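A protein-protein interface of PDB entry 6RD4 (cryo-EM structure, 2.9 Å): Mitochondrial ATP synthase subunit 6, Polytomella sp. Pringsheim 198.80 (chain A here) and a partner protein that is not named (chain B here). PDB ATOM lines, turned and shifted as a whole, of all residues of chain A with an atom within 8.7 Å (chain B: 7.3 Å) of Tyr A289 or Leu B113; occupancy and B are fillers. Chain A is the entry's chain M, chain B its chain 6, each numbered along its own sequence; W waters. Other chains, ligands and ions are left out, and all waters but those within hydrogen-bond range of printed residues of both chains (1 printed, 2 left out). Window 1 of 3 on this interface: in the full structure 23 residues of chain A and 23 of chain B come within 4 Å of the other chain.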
ATOM      1  N   ILE A 160       1.422 -19.592 -18.388  1.00  0.00           N
ATOM      2  CA  ILE A 160       0.269 -20.136 -19.072  1.00  0.00           C
ATOM      3  C   ILE A 160       0.588 -21.470 -19.713  1.00  0.00           C
ATOM      4  O   ILE A 160      -0.306 -22.284 -19.883  1.00  0.00           O
ATOM      5  CB  ILE A 160      -0.294 -19.119 -20.080  1.00  0.00           C
ATOM      6  CG1 ILE A 160      -1.766 -19.393 -20.320  1.00  0.00           C
ATOM      7  CG2 ILE A 160       0.435 -19.136 -21.372  1.00  0.00           C
ATOM      8  CD1 ILE A 160      -2.413 -18.432 -21.220  1.00  0.00           C
ATOM      9  N   ASN A 163       0.467 -23.621 -16.385  1.00  0.00           N
ATOM     10  CA  ASN A 163      -0.871 -23.732 -15.821  1.00  0.00           C
ATOM     11  C   ASN A 163      -1.756 -24.612 -16.673  1.00  0.00           C
ATOM     12  O   ASN A 163      -2.597 -25.340 -16.149  1.00  0.00           O
ATOM     13  CB  ASN A 163      -1.516 -22.365 -15.696  1.00  0.00           C
ATOM     14  CG  ASN A 163      -0.937 -21.550 -14.610  1.00  0.00           C
ATOM     15  OD1 ASN A 163      -1.222 -20.373 -14.501  1.00  0.00           O
ATOM     16  ND2 ASN A 163      -0.135 -22.158 -13.783  1.00  0.00           N
ATOM     17  N   LEU A 164      -1.598 -24.547 -17.983  1.00  0.00           N
ATOM     18  CA  LEU A 164      -2.407 -25.359 -18.865  1.00  0.00           C
ATOM     19  C   LEU A 164      -1.903 -26.777 -18.989  1.00  0.00           C
ATOM     20  O   LEU A 164      -2.610 -27.599 -19.564  1.00  0.00           O
ATOM     21  CB  LEU A 164      -2.479 -24.748 -20.254  1.00  0.00           C
ATOM     22  CG  LEU A 164      -3.278 -23.481 -20.509  1.00  0.00           C
ATOM     23  CD1 LEU A 164      -3.110 -23.137 -21.943  1.00  0.00           C
ATOM     24  CD2 LEU A 164      -4.719 -23.634 -20.179  1.00  0.00           C
ATOM     25  N   LEU A 165      -0.701 -27.086 -18.511  1.00  0.00           N
ATOM     26  CA  LEU A 165      -0.323 -28.486 -18.390  1.00  0.00           C
ATOM     27  C   LEU A 165      -1.178 -29.209 -17.382  1.00  0.00           C
ATOM     28  O   LEU A 165      -1.462 -30.386 -17.565  1.00  0.00           O
ATOM     29  CB  LEU A 165       1.125 -28.652 -17.984  1.00  0.00           C
ATOM     30  CG  LEU A 165       2.189 -28.547 -19.030  1.00  0.00           C
ATOM     31  CD1 LEU A 165       3.506 -28.625 -18.335  1.00  0.00           C
ATOM     32  CD2 LEU A 165       1.998 -29.718 -19.919  1.00  0.00           C
ATOM     33  N   GLY A 166      -1.622 -28.526 -16.336  1.00  0.00           N
ATOM     34  CA  GLY A 166      -2.459 -29.147 -15.339  1.00  0.00           C
ATOM     35  C   GLY A 166      -3.813 -29.570 -15.836  1.00  0.00           C
ATOM     36  O   GLY A 166      -4.474 -30.366 -15.167  1.00  0.00           O
ATOM     37  N   LEU A 167      -4.229 -29.074 -16.990  1.00  0.00           N
ATOM     38  CA  LEU A 167      -5.491 -29.410 -17.614  1.00  0.00           C
ATOM     39  C   LEU A 167      -5.334 -30.382 -18.766  1.00  0.00           C
ATOM     40  O   LEU A 167      -6.330 -30.770 -19.367  1.00  0.00           O
ATOM     41  CB  LEU A 167      -6.163 -28.136 -18.090  1.00  0.00           C
ATOM     42  CG  LEU A 167      -6.227 -27.168 -16.932  1.00  0.00           C
ATOM     43  CD1 LEU A 167      -6.358 -25.817 -17.470  1.00  0.00           C
ATOM     44  CD2 LEU A 167      -7.420 -27.500 -16.111  1.00  0.00           C
ATOM     45  N   MET A 168      -4.133 -30.757 -19.097  1.00  0.00           N
ATOM     46  CA  MET A 168      -3.936 -31.870 -19.994  1.00  0.00           C
ATOM     47  C   MET A 168      -4.052 -33.166 -19.213  1.00  0.00           C
ATOM     48  O   MET A 168      -3.696 -33.213 -18.039  1.00  0.00           O
ATOM     49  CB  MET A 168      -2.573 -31.794 -20.660  1.00  0.00           C
ATOM     50  CG  MET A 168      -2.376 -30.591 -21.523  1.00  0.00           C
ATOM     51  SD  MET A 168      -3.675 -30.402 -22.736  1.00  0.00           S
ATOM     52  CE  MET A 168      -4.422 -28.871 -22.210  1.00  0.00           C
ATOM     53  N   PRO A 169      -4.584 -34.216 -19.820  1.00  0.00           N
ATOM     54  CA  PRO A 169      -4.647 -35.499 -19.131  1.00  0.00           C
ATOM     55  C   PRO A 169      -3.268 -36.078 -18.895  1.00  0.00           C
ATOM     56  O   PRO A 169      -2.336 -35.836 -19.657  1.00  0.00           O
ATOM     57  CB  PRO A 169      -5.468 -36.367 -20.082  1.00  0.00           C
ATOM     58  CG  PRO A 169      -5.487 -35.659 -21.331  1.00  0.00           C
ATOM     59  CD  PRO A 169      -5.406 -34.231 -21.032  1.00  0.00           C
ATOM     60  N   PHE A 170      -3.154 -36.817 -17.794  1.00  0.00           N
ATOM     61  CA  PHE A 170      -1.958 -37.446 -17.242  1.00  0.00           C
ATOM     62  C   PHE A 170      -0.914 -36.454 -16.780  1.00  0.00           C
ATOM     63  O   PHE A 170       0.204 -36.852 -16.478  1.00  0.00           O
ATOM     64  CB  PHE A 170      -1.308 -38.437 -18.212  1.00  0.00           C
ATOM     65  CG  PHE A 170      -2.255 -39.431 -18.781  1.00  0.00           C
ATOM     66  CD1 PHE A 170      -2.583 -40.567 -18.079  1.00  0.00           C
ATOM     67  CD2 PHE A 170      -2.812 -39.236 -20.020  1.00  0.00           C
ATOM     68  CE1 PHE A 170      -3.460 -41.472 -18.598  1.00  0.00           C
ATOM     69  CE2 PHE A 170      -3.684 -40.141 -20.541  1.00  0.00           C
ATOM     70  CZ  PHE A 170      -4.004 -41.261 -19.828  1.00  0.00           C
ATOM     71  N   MET A 244      -3.462 -22.718  -8.273  1.00  0.00           N
ATOM     72  CA  MET A 244      -3.237 -23.944  -9.011  1.00  0.00           C
ATOM     73  C   MET A 244      -3.347 -25.154  -8.122  1.00  0.00           C
ATOM     74  O   MET A 244      -3.585 -26.250  -8.621  1.00  0.00           O
ATOM     75  CB  MET A 244      -1.874 -23.913  -9.684  1.00  0.00           C
ATOM     76  CG  MET A 244      -1.764 -22.918 -10.796  1.00  0.00           C
ATOM     77  SD  MET A 244      -2.846 -23.302 -12.165  1.00  0.00           S
ATOM     78  CE  MET A 244      -3.983 -21.947 -12.040  1.00  0.00           C
ATOM     79  N   SER A 282     -17.539 -31.296 -14.322  1.00  0.00           N
ATOM     80  CA  SER A 282     -17.202 -30.728 -15.614  1.00  0.00           C
ATOM     81  C   SER A 282     -17.159 -29.214 -15.600  1.00  0.00           C
ATOM     82  O   SER A 282     -16.387 -28.631 -16.355  1.00  0.00           O
ATOM     83  CB  SER A 282     -18.206 -31.191 -16.641  1.00  0.00           C
ATOM     84  OG  SER A 282     -18.135 -32.590 -16.800  1.00  0.00           O
ATOM     85  N   ALA A 283     -17.971 -28.566 -14.781  1.00  0.00           N
ATOM     86  CA  ALA A 283     -17.928 -27.119 -14.697  1.00  0.00           C
ATOM     87  C   ALA A 283     -16.834 -26.614 -13.778  1.00  0.00           C
ATOM     88  O   ALA A 283     -16.598 -25.409 -13.741  1.00  0.00           O
ATOM     89  CB  ALA A 283     -19.268 -26.572 -14.233  1.00  0.00           C
ATOM     90  N   LEU A 284     -16.174 -27.484 -13.027  1.00  0.00           N
ATOM     91  CA  LEU A 284     -15.003 -27.062 -12.273  1.00  0.00           C
ATOM     92  C   LEU A 284     -13.721 -27.209 -13.062  1.00  0.00           C
ATOM     93  O   LEU A 284     -12.772 -26.467 -12.814  1.00  0.00           O
ATOM     94  CB  LEU A 284     -14.863 -27.861 -10.985  1.00  0.00           C
ATOM     95  CG  LEU A 284     -15.845 -27.526  -9.884  1.00  0.00           C
ATOM     96  CD1 LEU A 284     -15.642 -28.509  -8.769  1.00  0.00           C
ATOM     97  CD2 LEU A 284     -15.655 -26.109  -9.403  1.00  0.00           C
ATOM     98  N   VAL A 285     -13.650 -28.171 -13.978  1.00  0.00           N
ATOM     99  CA  VAL A 285     -12.533 -28.202 -14.906  1.00  0.00           C
ATOM    100  C   VAL A 285     -12.632 -27.037 -15.871  1.00  0.00           C
ATOM    101  O   VAL A 285     -11.616 -26.517 -16.333  1.00  0.00           O
ATOM    102  CB  VAL A 285     -12.477 -29.550 -15.635  1.00  0.00           C
ATOM    103  CG1 VAL A 285     -11.175 -29.712 -16.374  1.00  0.00           C
ATOM    104  CG2 VAL A 285     -12.597 -30.637 -14.656  1.00  0.00           C
ATOM    105  N   GLY A 286     -13.843 -26.585 -16.175  1.00  0.00           N
ATOM    106  CA  GLY A 286     -13.989 -25.425 -17.027  1.00  0.00           C
ATOM    107  C   GLY A 286     -13.608 -24.135 -16.345  1.00  0.00           C
ATOM    108  O   GLY A 286     -13.104 -23.222 -16.989  1.00  0.00           O
ATOM    109  N   LEU A 287     -13.855 -24.032 -15.046  1.00  0.00           N
ATOM    110  CA  LEU A 287     -13.386 -22.876 -14.301  1.00  0.00           C
ATOM    111  C   LEU A 287     -11.879 -22.907 -14.154  1.00  0.00           C
ATOM    112  O   LEU A 287     -11.238 -21.858 -14.082  1.00  0.00           O
ATOM    113  CB  LEU A 287     -14.066 -22.837 -12.938  1.00  0.00           C
ATOM    114  CG  LEU A 287     -13.604 -21.873 -11.854  1.00  0.00           C
ATOM    115  CD1 LEU A 287     -13.769 -20.473 -12.332  1.00  0.00           C
ATOM    116  CD2 LEU A 287     -14.391 -22.089 -10.601  1.00  0.00           C
ATOM    117  N   GLU A 288     -11.298 -24.096 -14.135  1.00  0.00           N
ATOM    118  CA  GLU A 288      -9.857 -24.223 -14.029  1.00  0.00           C
ATOM    119  C   GLU A 288      -9.146 -23.807 -15.298  1.00  0.00           C
ATOM    120  O   GLU A 288      -7.960 -23.492 -15.254  1.00  0.00           O
ATOM    121  CB  GLU A 288      -9.498 -25.650 -13.703  1.00  0.00           C
ATOM    122  CG  GLU A 288      -9.530 -25.972 -12.269  1.00  0.00           C
ATOM    123  CD  GLU A 288      -9.017 -27.345 -12.042  1.00  0.00           C
ATOM    124  OE1 GLU A 288      -8.040 -27.737 -12.703  1.00  0.00           O
ATOM    125  OE2 GLU A 288      -9.603 -28.051 -11.213  1.00  0.00           O
ATOM    126  N   TYR A 289      -9.824 -23.855 -16.440  1.00  0.00           N
ATOM    127  CA  TYR A 289      -9.253 -23.293 -17.654  1.00  0.00           C
ATOM    128  C   TYR A 289      -9.273 -21.788 -17.613  1.00  0.00           C
ATOM    129  O   TYR A 289      -8.502 -21.140 -18.313  1.00  0.00           O
ATOM    130  CB  TYR A 289     -10.028 -23.751 -18.871  1.00  0.00           C
ATOM    131  CG  TYR A 289      -9.539 -25.003 -19.496  1.00  0.00           C
ATOM    132  CD1 TYR A 289      -8.535 -24.977 -20.426  1.00  0.00           C
ATOM    133  CD2 TYR A 289     -10.101 -26.213 -19.165  1.00  0.00           C
ATOM    134  CE1 TYR A 289      -8.095 -26.121 -21.005  1.00  0.00           C
ATOM    135  CE2 TYR A 289      -9.666 -27.359 -19.732  1.00  0.00           C
ATOM    136  CZ  TYR A 289      -8.670 -27.310 -20.653  1.00  0.00           C
ATOM    137  OH  TYR A 289      -8.234 -28.466 -21.225  1.00  0.00           O
ATOM    138  N   LEU A 290     -10.188 -21.219 -16.855  1.00  0.00           N
ATOM    139  CA  LEU A 290     -10.263 -19.778 -16.727  1.00  0.00           C
ATOM    140  C   LEU A 290      -9.256 -19.277 -15.717  1.00  0.00           C
ATOM    141  O   LEU A 290      -8.656 -18.225 -15.912  1.00  0.00           O
ATOM    142  CB  LEU A 290     -11.674 -19.385 -16.326  1.00  0.00           C
ATOM    143  CG  LEU A 290     -12.155 -17.993 -16.675  1.00  0.00           C
ATOM    144  CD1 LEU A 290     -11.951 -17.741 -18.137  1.00  0.00           C
ATOM    145  CD2 LEU A 290     -13.603 -17.914 -16.327  1.00  0.00           C
ATOM    146  N   VAL A 291      -9.035 -20.033 -14.649  1.00  0.00           N
ATOM    147  CA  VAL A 291      -8.050 -19.660 -13.646  1.00  0.00           C
ATOM    148  C   VAL A 291      -6.633 -19.895 -14.159  1.00  0.00           C
ATOM    149  O   VAL A 291      -5.704 -19.182 -13.780  1.00  0.00           O
ATOM    150  CB  VAL A 291      -8.390 -20.428 -12.359  1.00  0.00           C
ATOM    151  CG1 VAL A 291      -7.331 -20.325 -11.316  1.00  0.00           C
ATOM    152  CG2 VAL A 291      -9.673 -19.891 -11.801  1.00  0.00           C
ATOM    153  N   ALA A 292      -6.450 -20.846 -15.072  1.00  0.00           N
ATOM    154  CA  ALA A 292      -5.144 -21.067 -15.678  1.00  0.00           C
ATOM    155  C   ALA A 292      -4.723 -19.897 -16.545  1.00  0.00           C
ATOM    156  O   ALA A 292      -3.545 -19.543 -16.582  1.00  0.00           O
ATOM    157  CB  ALA A 292      -5.163 -22.337 -16.512  1.00  0.00           C
ATOM    158  N   VAL A 293      -5.668 -19.284 -17.245  1.00  0.00           N
ATOM    159  CA  VAL A 293      -5.355 -18.159 -18.110  1.00  0.00           C
ATOM    160  C   VAL A 293      -5.337 -16.864 -17.319  1.00  0.00           C
ATOM    161  O   VAL A 293      -4.543 -15.970 -17.602  1.00  0.00           O
ATOM    162  CB  VAL A 293      -6.355 -18.119 -19.277  1.00  0.00           C
ATOM    163  CG1 VAL A 293      -6.056 -17.004 -20.233  1.00  0.00           C
ATOM    164  CG2 VAL A 293      -6.308 -19.405 -20.021  1.00  0.00           C
ATOM    165  N   LEU A 294      -6.181 -16.744 -16.301  1.00  0.00           N
ATOM    166  CA  LEU A 294      -6.213 -15.506 -15.535  1.00  0.00           C
ATOM    167  C   LEU A 294      -5.000 -15.369 -14.644  1.00  0.00           C
ATOM    168  O   LEU A 294      -4.458 -14.277 -14.515  1.00  0.00           O
ATOM    169  CB  LEU A 294      -7.472 -15.425 -14.693  1.00  0.00           C
ATOM    170  CG  LEU A 294      -8.761 -14.988 -15.365  1.00  0.00           C
ATOM    171  CD1 LEU A 294      -9.761 -14.704 -14.306  1.00  0.00           C
ATOM    172  CD2 LEU A 294      -8.553 -13.783 -16.227  1.00  0.00           C
ATOM    173  N   GLN A 295      -4.555 -16.448 -14.015  1.00  0.00           N
ATOM    174  CA  GLN A 295      -3.444 -16.316 -13.088  1.00  0.00           C
ATOM    175  C   GLN A 295      -2.108 -16.165 -13.789  1.00  0.00           C
ATOM    176  O   GLN A 295      -1.149 -15.719 -13.167  1.00  0.00           O
ATOM    177  CB  GLN A 295      -3.398 -17.500 -12.139  1.00  0.00           C
ATOM    178  CG  GLN A 295      -4.541 -17.549 -11.173  1.00  0.00           C
ATOM    179  CD  GLN A 295      -4.733 -16.272 -10.400  1.00  0.00           C
ATOM    180  OE1 GLN A 295      -3.778 -15.652  -9.945  1.00  0.00           O
ATOM    181  NE2 GLN A 295      -5.983 -15.875 -10.237  1.00  0.00           N
ATOM    182  N   SER A 296      -2.013 -16.536 -15.051  1.00  0.00           N
ATOM    183  CA  SER A 296      -0.829 -16.183 -15.806  1.00  0.00           C
ATOM    184  C   SER A 296      -0.893 -14.751 -16.284  1.00  0.00           C
ATOM    185  O   SER A 296       0.142 -14.153 -16.576  1.00  0.00           O
ATOM    186  CB  SER A 296      -0.672 -17.121 -16.979  1.00  0.00           C
ATOM    187  OG  SER A 296      -1.750 -16.981 -17.860  1.00  0.00           O
ATOM    188  N   LEU B 108     -11.844 -36.516 -16.890  1.00  0.00           N
ATOM    189  CA  LEU B 108     -12.438 -35.193 -16.776  1.00  0.00           C
ATOM    190  C   LEU B 108     -11.659 -34.160 -17.556  1.00  0.00           C
ATOM    191  O   LEU B 108     -12.243 -33.210 -18.073  1.00  0.00           O
ATOM    192  CB  LEU B 108     -12.497 -34.771 -15.324  1.00  0.00           C
ATOM    193  CG  LEU B 108     -13.743 -35.133 -14.563  1.00  0.00           C
ATOM    194  CD1 LEU B 108     -13.547 -34.692 -13.166  1.00  0.00           C
ATOM    195  CD2 LEU B 108     -14.860 -34.386 -15.177  1.00  0.00           C
ATOM    196  N   GLN B 109     -10.348 -34.311 -17.626  1.00  0.00           N
ATOM    197  CA  GLN B 109      -9.531 -33.352 -18.340  1.00  0.00           C
ATOM    198  C   GLN B 109      -9.598 -33.561 -19.837  1.00  0.00           C
ATOM    199  O   GLN B 109      -9.590 -32.585 -20.584  1.00  0.00           O
ATOM    200  CB  GLN B 109      -8.096 -33.444 -17.860  1.00  0.00           C
ATOM    201  CG  GLN B 109      -7.904 -32.886 -16.510  1.00  0.00           C
ATOM    202  CD  GLN B 109      -6.636 -33.352 -15.896  1.00  0.00           C
ATOM    203  OE1 GLN B 109      -5.962 -34.210 -16.427  1.00  0.00           O
ATOM    204  NE2 GLN B 109      -6.289 -32.780 -14.765  1.00  0.00           N
ATOM    205  N   ALA B 110      -9.664 -34.808 -20.295  1.00  0.00           N
ATOM    206  CA  ALA B 110      -9.802 -35.081 -21.714  1.00  0.00           C
ATOM    207  C   ALA B 110     -11.207 -34.871 -22.221  1.00  0.00           C
ATOM    208  O   ALA B 110     -11.420 -34.929 -23.427  1.00  0.00           O
ATOM    209  CB  ALA B 110      -9.387 -36.504 -22.043  1.00  0.00           C
ATOM    210  N   ALA B 111     -12.174 -34.668 -21.343  1.00  0.00           N
ATOM    211  CA  ALA B 111     -13.514 -34.366 -21.806  1.00  0.00           C
ATOM    212  C   ALA B 111     -13.596 -32.942 -22.307  1.00  0.00           C
ATOM    213  O   ALA B 111     -14.442 -32.625 -23.143  1.00  0.00           O
ATOM    214  CB  ALA B 111     -14.520 -34.592 -20.691  1.00  0.00           C
ATOM    215  N   TRP B 112     -12.742 -32.063 -21.793  1.00  0.00           N
ATOM    216  CA  TRP B 112     -12.715 -30.678 -22.234  1.00  0.00           C
ATOM    217  C   TRP B 112     -11.872 -30.480 -23.469  1.00  0.00           C
ATOM    218  O   TRP B 112     -12.100 -29.525 -24.204  1.00  0.00           O
ATOM    219  CB  TRP B 112     -12.192 -29.786 -21.128  1.00  0.00           C
ATOM    220  CG  TRP B 112     -13.237 -29.335 -20.244  1.00  0.00           C
ATOM    221  CD1 TRP B 112     -13.537 -29.838 -19.039  1.00  0.00           C
ATOM    222  CD2 TRP B 112     -14.163 -28.290 -20.489  1.00  0.00           C
ATOM    223  NE1 TRP B 112     -14.593 -29.173 -18.498  1.00  0.00           N
ATOM    224  CE2 TRP B 112     -14.997 -28.210 -19.378  1.00  0.00           C
ATOM    225  CE3 TRP B 112     -14.371 -27.416 -21.545  1.00  0.00           C
ATOM    226  CZ2 TRP B 112     -16.022 -27.294 -19.286  1.00  0.00           C
ATOM    227  CZ3 TRP B 112     -15.382 -26.505 -21.453  1.00  0.00           C
ATOM    228  CH2 TRP B 112     -16.196 -26.445 -20.332  1.00  0.00           C
ATOM    229  N   LEU B 113     -10.896 -31.341 -23.705  1.00  0.00           N
ATOM    230  CA  LEU B 113     -10.191 -31.338 -24.974  1.00  0.00           C
ATOM    231  C   LEU B 113     -11.102 -31.764 -26.106  1.00  0.00           C
ATOM    232  O   LEU B 113     -10.894 -31.369 -27.252  1.00  0.00           O
ATOM    233  CB  LEU B 113      -8.990 -32.266 -24.895  1.00  0.00           C
ATOM    234  CG  LEU B 113      -7.613 -31.746 -24.528  1.00  0.00           C
ATOM    235  CD1 LEU B 113      -7.610 -31.195 -23.171  1.00  0.00           C
ATOM    236  CD2 LEU B 113      -6.691 -32.911 -24.557  1.00  0.00           C
ATOM    237  N   ILE B 114     -12.094 -32.589 -25.810  1.00  0.00           N
ATOM    238  CA  ILE B 114     -13.072 -32.999 -26.803  1.00  0.00           C
ATOM    239  C   ILE B 114     -14.095 -31.899 -27.022  1.00  0.00           C
ATOM    240  O   ILE B 114     -14.489 -31.615 -28.154  1.00  0.00           O
ATOM    241  CB  ILE B 114     -13.697 -34.328 -26.347  1.00  0.00           C
ATOM    242  CG1 ILE B 114     -12.752 -35.471 -26.676  1.00  0.00           C
ATOM    243  CG2 ILE B 114     -15.057 -34.552 -26.921  1.00  0.00           C
ATOM    244  CD1 ILE B 114     -12.979 -36.665 -25.862  1.00  0.00           C
ATOM    245  N   SER B 115     -14.511 -31.233 -25.952  1.00  0.00           N
ATOM    246  CA  SER B 115     -15.488 -30.169 -26.082  1.00  0.00           C
ATOM    247  C   SER B 115     -14.889 -28.893 -26.632  1.00  0.00           C
ATOM    248  O   SER B 115     -15.635 -27.991 -27.001  1.00  0.00           O
ATOM    249  CB  SER B 115     -16.133 -29.883 -24.743  1.00  0.00           C
ATOM    250  OG  SER B 115     -16.848 -31.014 -24.309  1.00  0.00           O
ATOM    251  N   PHE B 116     -13.569 -28.782 -26.669  1.00  0.00           N
ATOM    252  CA  PHE B 116     -12.943 -27.628 -27.293  1.00  0.00           C
ATOM    253  C   PHE B 116     -12.775 -27.818 -28.784  1.00  0.00           C
ATOM    254  O   PHE B 116     -12.761 -26.840 -29.525  1.00  0.00           O
ATOM    255  CB  PHE B 116     -11.598 -27.352 -26.646  1.00  0.00           C
ATOM    256  CG  PHE B 116     -11.696 -26.580 -25.380  1.00  0.00           C
ATOM    257  CD1 PHE B 116     -12.789 -25.791 -25.123  1.00  0.00           C
ATOM    258  CD2 PHE B 116     -10.698 -26.650 -24.443  1.00  0.00           C
ATOM    259  CE1 PHE B 116     -12.872 -25.080 -23.958  1.00  0.00           C
ATOM    260  CE2 PHE B 116     -10.790 -25.952 -23.282  1.00  0.00           C
ATOM    261  CZ  PHE B 116     -11.873 -25.161 -23.041  1.00  0.00           C
ATOM    262  N   SER B 117     -12.674 -29.058 -29.252  1.00  0.00           N
ATOM    263  CA  SER B 117     -12.675 -29.302 -30.683  1.00  0.00           C
ATOM    264  C   SER B 117     -14.043 -29.103 -31.299  1.00  0.00           C
ATOM    265  O   SER B 117     -14.150 -29.017 -32.521  1.00  0.00           O
ATOM    266  CB  SER B 117     -12.213 -30.716 -30.972  1.00  0.00           C
ATOM    267  OG  SER B 117     -11.023 -30.991 -30.276  1.00  0.00           O
ATOM    268  N   SER B 118     -15.086 -29.046 -30.492  1.00  0.00           N
ATOM    269  CA  SER B 118     -16.441 -28.960 -30.982  1.00  0.00           C
ATOM    270  C   SER B 118     -17.107 -27.641 -30.667  1.00  0.00           C
ATOM    271  O   SER B 118     -18.277 -27.467 -31.001  1.00  0.00           O
ATOM    272  CB  SER B 118     -17.279 -30.096 -30.398  1.00  0.00           C
ATOM    273  OG  SER B 118     -17.081 -31.291 -31.133  1.00  0.00           O
HETATM  274  O   HOH W   1      -8.107 -30.501 -14.243  1.00  0.00           O
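The backbone carbonyl oxygen (O) of Gly A166 is in hydrogen-bond range of the side-chain amide nitrogen (NE2) of Gln B109, at 3.0 Å. The side-chain amide oxygen (OE1) of Gln B109 lies close to the backbone carbonyl oxygen (O) of Met A168, at 3.0 Å. O of Ser A282 is in hydrogen-bond range of NE1 of Trp B112 (2.8 Å).
OG of Ser B117 is in hydrogen-bond range of O of Leu B113.
Among the printed residues, pairs that only touch across the chains: Pro A169 with Gln B109 (3.3 Å), Tyr A289 with Leu B113 (3.4 Å), Tyr A289 with Phe B116 (3.5 Å), Leu A167 with Gln B109 (3.5 Å), Gly A286 with Trp B112 (3.6 Å), Val A285 with Trp B112 (3.6 Å), Tyr A289 with Trp B112 (3.8 Å) and Pro A169 with Leu B113 (3.98 Å).
Printed residues of chain B within 4 Å of Leu A167: Gln B109 (3.5 Å). Met A244 touches none of the printed residues of chain B. Printed residues of chain B within 4 Å of Ser A282: Trp B112 (2.8 Å). Of the printed residues of chain B, Gly A286 touches Trp B112 (3.6 Å). Tyr A289 touches just these residues of chain B: Trp B112, Leu B113 and Phe B116. Of the printed residues of chain A, Leu B113 touches Pro A169 (3.98 Å) and Tyr A289 (3.4 Å). Printed residues of chain A within 4 Å of Phe B116: Tyr A289 (3.5 Å). The nearest printed residue of chain B that does not touch Gly A286 is Phe B116 (6.4 Å).
Hydrophobic or aromatic side chains of chain B within 4 Å of the printed part of chain A: Trp B112, Leu B113 and Phe B116. Of the 25 printed residues of chain A, 8 touch a printed residue of chain B. Hydrophobic or aromatic side chains of chain A that line the printed part of chain B: Pro A169, Val A285 and Tyr A289. Among the printed residues, 11 pairs touch across the chains.
Water W1 bridges NE2 of Gln B109 (3.0 Å) and OE1 of Glu A288 (3.2 Å).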
